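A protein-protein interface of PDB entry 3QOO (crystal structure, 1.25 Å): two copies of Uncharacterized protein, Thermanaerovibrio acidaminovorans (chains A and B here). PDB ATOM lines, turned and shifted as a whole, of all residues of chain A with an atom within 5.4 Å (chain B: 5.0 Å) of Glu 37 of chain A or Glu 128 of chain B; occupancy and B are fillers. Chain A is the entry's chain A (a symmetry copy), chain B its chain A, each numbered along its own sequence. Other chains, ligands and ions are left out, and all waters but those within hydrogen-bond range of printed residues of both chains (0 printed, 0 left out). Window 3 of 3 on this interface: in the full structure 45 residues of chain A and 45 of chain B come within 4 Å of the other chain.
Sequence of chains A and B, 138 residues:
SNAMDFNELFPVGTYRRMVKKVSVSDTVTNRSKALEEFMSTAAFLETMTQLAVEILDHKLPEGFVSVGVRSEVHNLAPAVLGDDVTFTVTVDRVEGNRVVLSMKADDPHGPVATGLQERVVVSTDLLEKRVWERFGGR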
ATOM      1  N   VAL A  22      29.156  34.377  11.832  1.00  0.00           N
ATOM      2  CA  VAL A  22      28.802  33.003  11.452  1.00  0.00           C
ATOM      3  C   VAL A  22      27.362  32.988  10.967  1.00  0.00           C
ATOM      4  O   VAL A  22      26.429  33.287  11.720  1.00  0.00           O
ATOM      5  CB  VAL A  22      29.029  32.004  12.591  1.00  0.00           C
ATOM      6  CG1 VAL A  22      28.639  30.600  12.148  1.00  0.00           C
ATOM      7  CG2 VAL A  22      30.463  32.064  13.113  1.00  0.00           C
ATOM      8  N   THR A  27      27.906  27.078   7.917  1.00  0.00           N
ATOM      9  CA  THR A  27      27.673  25.899   8.763  1.00  0.00           C
ATOM     10  C   THR A  27      27.231  24.735   7.913  1.00  0.00           C
ATOM     11  O   THR A  27      27.435  23.557   8.296  1.00  0.00           O
ATOM     12  CB  THR A  27      26.602  26.145   9.836  1.00  0.00           C
ATOM     13  OG1 THR A  27      25.303  26.257   9.211  1.00  0.00           O
ATOM     14  CG2 THR A  27      26.897  27.347  10.686  1.00  0.00           C
ATOM     15  N   ALA A  34      23.240  17.588  11.882  1.00  0.00           N
ATOM     16  CA  ALA A  34      23.488  17.672  13.329  1.00  0.00           C
ATOM     17  C   ALA A  34      24.460  18.803  13.710  1.00  0.00           C
ATOM     18  O   ALA A  34      24.491  19.229  14.868  1.00  0.00           O
ATOM     19  CB  ALA A  34      24.052  16.353  13.817  1.00  0.00           C
ATOM     20  N   LEU A  35      25.272  19.278  12.764  1.00  0.00           N
ATOM     21  CA  LEU A  35      26.290  20.291  13.049  1.00  0.00           C
ATOM     22  C   LEU A  35      25.923  21.663  12.519  1.00  0.00           C
ATOM     23  O   LEU A  35      26.795  22.491  12.351  1.00  0.00           O
ATOM     24  CB  LEU A  35      27.610  19.818  12.453  1.00  0.00           C
ATOM     25  CG  LEU A  35      28.014  18.396  12.877  1.00  0.00           C
ATOM     26  CD1 LEU A  35      29.385  18.078  12.362  1.00  0.00           C
ATOM     27  CD2 LEU A  35      27.929  18.224  14.425  1.00  0.00           C
ATOM     28  N   GLU A  36      24.635  21.923  12.335  1.00  0.00           N
ATOM     29  CA  GLU A  36      24.170  23.157  11.754  1.00  0.00           C
ATOM     30  C   GLU A  36      24.374  24.373  12.654  1.00  0.00           C
ATOM     31  O   GLU A  36      24.201  25.491  12.182  1.00  0.00           O
ATOM     32  CB  GLU A  36      22.662  23.052  11.530  1.00  0.00           C
ATOM     33  CG  GLU A  36      22.128  22.091  10.533  1.00  0.00           C
ATOM     34  CD  GLU A  36      20.593  22.117  10.568  1.00  0.00           C
ATOM     35  OE1 GLU A  36      19.970  21.693  11.583  1.00  0.00           O
ATOM     36  OE2 GLU A  36      19.999  22.569   9.581  1.00  0.00           O
ATOM     37  N   GLU A  37      24.697  24.182  13.925  1.00  0.00           N
ATOM     38  CA  GLU A  37      24.784  25.292  14.874  1.00  0.00           C
ATOM     39  C   GLU A  37      26.107  26.038  14.822  1.00  0.00           C
ATOM     40  O   GLU A  37      26.187  27.106  15.385  1.00  0.00           O
ATOM     41  CB  GLU A  37      24.532  24.856  16.331  1.00  0.00           C
ATOM     42  CG  GLU A  37      23.088  24.833  16.702  1.00  0.00           C
ATOM     43  CD  GLU A  37      22.808  24.700  18.183  1.00  0.00           C
ATOM     44  OE1 GLU A  37      23.284  25.516  18.999  1.00  0.00           O
ATOM     45  OE2 GLU A  37      22.010  23.837  18.538  1.00  0.00           O
ATOM     46  N   PHE A  38      27.140  25.505  14.203  1.00  0.00           N
ATOM     47  CA  PHE A  38      28.442  26.162  14.291  1.00  0.00           C
ATOM     48  C   PHE A  38      29.249  26.089  13.015  1.00  0.00           C
ATOM     49  O   PHE A  38      28.986  25.296  12.114  1.00  0.00           O
ATOM     50  CB  PHE A  38      29.206  25.619  15.499  1.00  0.00           C
ATOM     51  CG  PHE A  38      29.355  24.117  15.522  1.00  0.00           C
ATOM     52  CD1 PHE A  38      30.413  23.508  14.877  1.00  0.00           C
ATOM     53  CD2 PHE A  38      28.476  23.348  16.254  1.00  0.00           C
ATOM     54  CE1 PHE A  38      30.574  22.157  14.943  1.00  0.00           C
ATOM     55  CE2 PHE A  38      28.619  21.994  16.320  1.00  0.00           C
ATOM     56  CZ  PHE A  38      29.658  21.385  15.671  1.00  0.00           C
ATOM     57  N   MET A  39      30.241  26.959  12.944  1.00  0.00           N
ATOM     58  CA  MET A  39      31.015  27.158  11.734  1.00  0.00           C
ATOM     59  C   MET A  39      31.808  25.910  11.359  1.00  0.00           C
ATOM     60  O   MET A  39      32.426  25.268  12.215  1.00  0.00           O
ATOM     61  CB  MET A  39      31.968  28.335  11.967  1.00  0.00           C
ATOM     62  CG  MET A  39      32.857  28.692  10.762  1.00  0.00           C
ATOM     63  SD  MET A  39      33.820  30.383  10.978  1.00  0.00           S
ATOM     64  CE  MET A  39      32.618  31.205   9.930  1.00  0.00           C
ATOM     65  N   ALA A  79      32.162  27.832  17.126  1.00  0.00           N
ATOM     66  CA  ALA A  79      31.777  29.211  16.811  1.00  0.00           C
ATOM     67  C   ALA A  79      30.333  29.152  16.326  1.00  0.00           C
ATOM     68  O   ALA A  79      30.064  28.780  15.189  1.00  0.00           O
ATOM     69  CB  ALA A  79      32.711  29.805  15.757  1.00  0.00           C
ATOM     70  N   VAL A  80      29.404  29.475  17.209  1.00  0.00           N
ATOM     71  CA  VAL A  80      27.985  29.292  16.929  1.00  0.00           C
ATOM     72  C   VAL A  80      27.474  30.308  15.887  1.00  0.00           C
ATOM     73  O   VAL A  80      28.011  31.409  15.726  1.00  0.00           O
ATOM     74  CB  VAL A  80      27.191  29.471  18.295  1.00  0.00           C
ATOM     75  CG1 VAL A  80      27.183  30.912  18.769  1.00  0.00           C
ATOM     76  CG2 VAL A  80      25.764  28.921  18.246  1.00  0.00           C
ATOM     77  N   LEU A  81      26.380  29.941  15.222  1.00  0.00           N
ATOM     78  CA  LEU A  81      25.655  30.891  14.406  1.00  0.00           C
ATOM     79  C   LEU A  81      25.460  32.201  15.183  1.00  0.00           C
ATOM     80  O   LEU A  81      25.064  32.190  16.343  1.00  0.00           O
ATOM     81  CB  LEU A  81      24.269  30.363  14.100  1.00  0.00           C
ATOM     82  CG  LEU A  81      24.180  29.310  13.046  1.00  0.00           C
ATOM     83  CD1 LEU A  81      22.823  28.596  13.259  1.00  0.00           C
ATOM     84  CD2 LEU A  81      24.288  29.934  11.661  1.00  0.00           C
ATOM     85  N   SER B 123      28.436  12.740  21.783  1.00  0.00           N
ATOM     86  CA  SER B 123      27.029  12.743  22.107  1.00  0.00           C
ATOM     87  C   SER B 123      26.405  14.051  21.635  1.00  0.00           C
ATOM     88  O   SER B 123      26.918  15.128  21.947  1.00  0.00           O
ATOM     89  CB  SER B 123      26.871  12.677  23.621  1.00  0.00           C
ATOM     90  OG  SER B 123      25.600  13.121  24.028  1.00  0.00           O
ATOM     91  N   THR B 124      25.325  13.977  20.875  1.00  0.00           N
ATOM     92  CA  THR B 124      24.639  15.175  20.386  1.00  0.00           C
ATOM     93  C   THR B 124      24.163  16.002  21.593  1.00  0.00           C
ATOM     94  O   THR B 124      24.206  17.226  21.563  1.00  0.00           O
ATOM     95  CB  THR B 124      23.470  14.847  19.439  1.00  0.00           C
ATOM     96  OG1 THR B 124      22.499  14.128  20.163  1.00  0.00           O
ATOM     97  CG2 THR B 124      23.966  14.019  18.283  1.00  0.00           C
ATOM     98  N   ASP B 125      23.687  15.332  22.650  1.00  0.00           N
ATOM     99  CA  ASP B 125      23.254  16.082  23.841  1.00  0.00           C
ATOM    100  C   ASP B 125      24.388  16.875  24.483  1.00  0.00           C
ATOM    101  O   ASP B 125      24.247  18.049  24.807  1.00  0.00           O
ATOM    102  CB  ASP B 125      22.615  15.127  24.874  1.00  0.00           C
ATOM    103  CG  ASP B 125      21.232  14.593  24.439  1.00  0.00           C
ATOM    104  OD1 ASP B 125      20.608  15.121  23.475  1.00  0.00           O
ATOM    105  OD2 ASP B 125      20.757  13.631  25.072  1.00  0.00           O
ATOM    106  N   LEU B 126      25.534  16.212  24.647  1.00  0.00           N
ATOM    107  CA  LEU B 126      26.664  16.882  25.246  1.00  0.00           C
ATOM    108  C   LEU B 126      27.209  17.981  24.345  1.00  0.00           C
ATOM    109  O   LEU B 126      27.639  19.021  24.852  1.00  0.00           O
ATOM    110  CB  LEU B 126      27.741  15.882  25.645  1.00  0.00           C
ATOM    111  CG  LEU B 126      27.372  14.872  26.718  1.00  0.00           C
ATOM    112  CD1 LEU B 126      28.568  13.954  27.029  1.00  0.00           C
ATOM    113  CD2 LEU B 126      26.816  15.529  27.983  1.00  0.00           C
ATOM    114  N   LEU B 127      27.166  17.784  23.035  1.00  0.00           N
ATOM    115  CA  LEU B 127      27.590  18.809  22.082  1.00  0.00           C
ATOM    116  C   LEU B 127      26.706  20.062  22.230  1.00  0.00           C
ATOM    117  O   LEU B 127      27.199  21.184  22.303  1.00  0.00           O
ATOM    118  CB  LEU B 127      27.495  18.274  20.646  1.00  0.00           C
ATOM    119  CG  LEU B 127      27.803  19.249  19.527  1.00  0.00           C
ATOM    120  CD1 LEU B 127      29.205  19.807  19.638  1.00  0.00           C
ATOM    121  CD2 LEU B 127      27.595  18.601  18.165  1.00  0.00           C
ATOM    122  N   GLU B 128      25.397  19.850  22.306  1.00  0.00           N
ATOM    123  CA  GLU B 128      24.441  20.950  22.453  1.00  0.00           C
ATOM    124  C   GLU B 128      24.729  21.724  23.720  1.00  0.00           C
ATOM    125  O   GLU B 128      24.701  22.954  23.716  1.00  0.00           O
ATOM    126  CB  GLU B 128      23.004  20.405  22.464  1.00  0.00           C
ATOM    127  CG  GLU B 128      21.925  21.477  22.362  1.00  0.00           C
ATOM    128  CD  GLU B 128      21.773  22.038  20.983  1.00  0.00           C
ATOM    129  OE1 GLU B 128      21.723  21.238  20.015  1.00  0.00           O
ATOM    130  OE2 GLU B 128      21.659  23.268  20.876  1.00  0.00           O
ATOM    131  N   LYS B 129      25.044  21.008  24.790  1.00  0.00           N
ATOM    132  CA  LYS B 129      25.366  21.648  26.058  1.00  0.00           C
ATOM    133  C   LYS B 129      26.685  22.416  25.994  1.00  0.00           C
ATOM    134  O   LYS B 129      26.801  23.497  26.565  1.00  0.00           O
ATOM    135  CB  LYS B 129      25.366  20.651  27.198  1.00  0.00           C
ATOM    136  CG  LYS B 129      23.985  20.199  27.585  1.00  0.00           C
ATOM    137  CD  LYS B 129      23.963  19.488  28.913  1.00  0.00           C
ATOM    138  CE  LYS B 129      22.527  19.148  29.309  1.00  0.00           C
ATOM    139  NZ  LYS B 129      21.546  20.051  28.665  1.00  0.00           N
ATOM    140  N   ARG B 130      27.678  21.890  25.289  1.00  0.00           N
ATOM    141  CA  ARG B 130      28.940  22.606  25.130  1.00  0.00           C
ATOM    142  C   ARG B 130      28.693  23.965  24.498  1.00  0.00           C
ATOM    143  O   ARG B 130      29.201  24.981  24.980  1.00  0.00           O
ATOM    144  CB  ARG B 130      29.940  21.805  24.278  1.00  0.00           C
ATOM    145  CG  ARG B 130      31.324  22.469  24.189  1.00  0.00           C
ATOM    146  CD  ARG B 130      32.371  21.712  23.407  1.00  0.00           C
ATOM    147  NE  ARG B 130      33.639  22.446  23.445  1.00  0.00           N
ATOM    148  CZ  ARG B 130      34.682  22.210  22.645  1.00  0.00           C
ATOM    149  NH1 ARG B 130      34.657  21.248  21.726  1.00  0.00           N
ATOM    150  NH2 ARG B 130      35.774  22.943  22.761  1.00  0.00           N
ATOM    151  N   VAL B 131      27.946  23.978  23.403  1.00  0.00           N
ATOM    152  CA  VAL B 131      27.654  25.203  22.671  1.00  0.00           C
ATOM    153  C   VAL B 131      26.900  26.161  23.571  1.00  0.00           C
ATOM    154  O   VAL B 131      27.186  27.348  23.619  1.00  0.00           O
ATOM    155  CB  VAL B 131      26.856  24.895  21.383  1.00  0.00           C
ATOM    156  CG1 VAL B 131      26.460  26.152  20.637  1.00  0.00           C
ATOM    157  CG2 VAL B 131      27.683  23.969  20.471  1.00  0.00           C
ATOM    158  N   TRP B 132      25.908  25.660  24.290  1.00  0.00           N
ATOM    159  CA  TRP B 132      25.119  26.488  25.206  1.00  0.00           C
ATOM    160  C   TRP B 132      26.012  27.130  26.254  1.00  0.00           C
ATOM    161  O   TRP B 132      25.922  28.331  26.512  1.00  0.00           O
ATOM    162  CB  TRP B 132      24.066  25.630  25.905  1.00  0.00           C
ATOM    163  CG  TRP B 132      23.305  26.350  26.978  1.00  0.00           C
ATOM    164  CD1 TRP B 132      23.505  26.296  28.325  1.00  0.00           C
ATOM    165  CD2 TRP B 132      22.253  27.285  26.760  1.00  0.00           C
ATOM    166  NE1 TRP B 132      22.614  27.138  28.965  1.00  0.00           N
ATOM    167  CE2 TRP B 132      21.843  27.759  28.025  1.00  0.00           C
ATOM    168  CE3 TRP B 132      21.605  27.770  25.613  1.00  0.00           C
ATOM    169  CZ2 TRP B 132      20.827  28.698  28.171  1.00  0.00           C
ATOM    170  CZ3 TRP B 132      20.611  28.695  25.754  1.00  0.00           C
ATOM    171  CH2 TRP B 132      20.218  29.148  27.031  1.00  0.00           C
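OE2 of Glu 128 of chain B lies close to OE2 of Glu 37 of chain A, at 2.4 Å.
The backbone carbonyl oxygen (O) of Glu 37 of chain A is in hydrogen-bond range of the backbone NH (N) of Leu 81 of chain A (2.8 Å).
Among the printed residues, merely in contact across the chains: Glu 37 of chain A with Val 131 of chain B, Val 80 of chain A with Val 131 of chain B, Leu 35 of chain A with Leu 127 of chain B and Phe 38 of chain A with Leu 127 of chain B.
No position is printed for both chains.
Of the 5 pairs that touch across the chains among the printed residues, none has its exchanged pair printed and touching as well.
Printed residues of chain A that touch a printed residue of chain B: Leu 35, Glu 37, Phe 38 and Val 80.
Hydrophobic or aromatic side chains of chain A within 4 Å of the printed part of chain B: Leu 35, Phe 38 and Val 80.
Of the 10 printed residues of chain B, 3 touch a printed residue of chain A.
Printed residues of chain B that touch a printed residue of chain A: Leu 127, Glu 128 and Val 131.
Among the printed residues, no Asp or Glu carboxylate lies within 4 Å of a Lys or Arg side-chain nitrogen of the other chain.
Of the printed residues of chain B, Glu 37 of chain A touches Glu 128 and Val 131.
Printed residues of chain A within 4 Å of Glu 128 of chain B: Glu 37 (2.4 Å).
Printed residues of chain B within 4 Å of Val 80 of chain A: Val 131.
Printed residues of chain A within 4 Å of Val 131 of chain B: Glu 37 (3.6 Å) and Val 80 (3.7 Å).
Printed residues of chain B within 4 Å of Phe 38 of chain A: Leu 127 (3.996 Å).
Of the printed residues of chain A, Leu 127 of chain B touches Leu 35 (3.8 Å) and Phe 38 (3.996 Å).
Printed residues of chain B within 4 Å of Leu 35 of chain A: Leu 127 (3.8 Å).
Glu 36 of chain A touches none of the printed residues of chain B.
The nearest printed residue of chain B that does not touch Phe 38 of chain A is Val 131 of chain B (4.3 Å).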
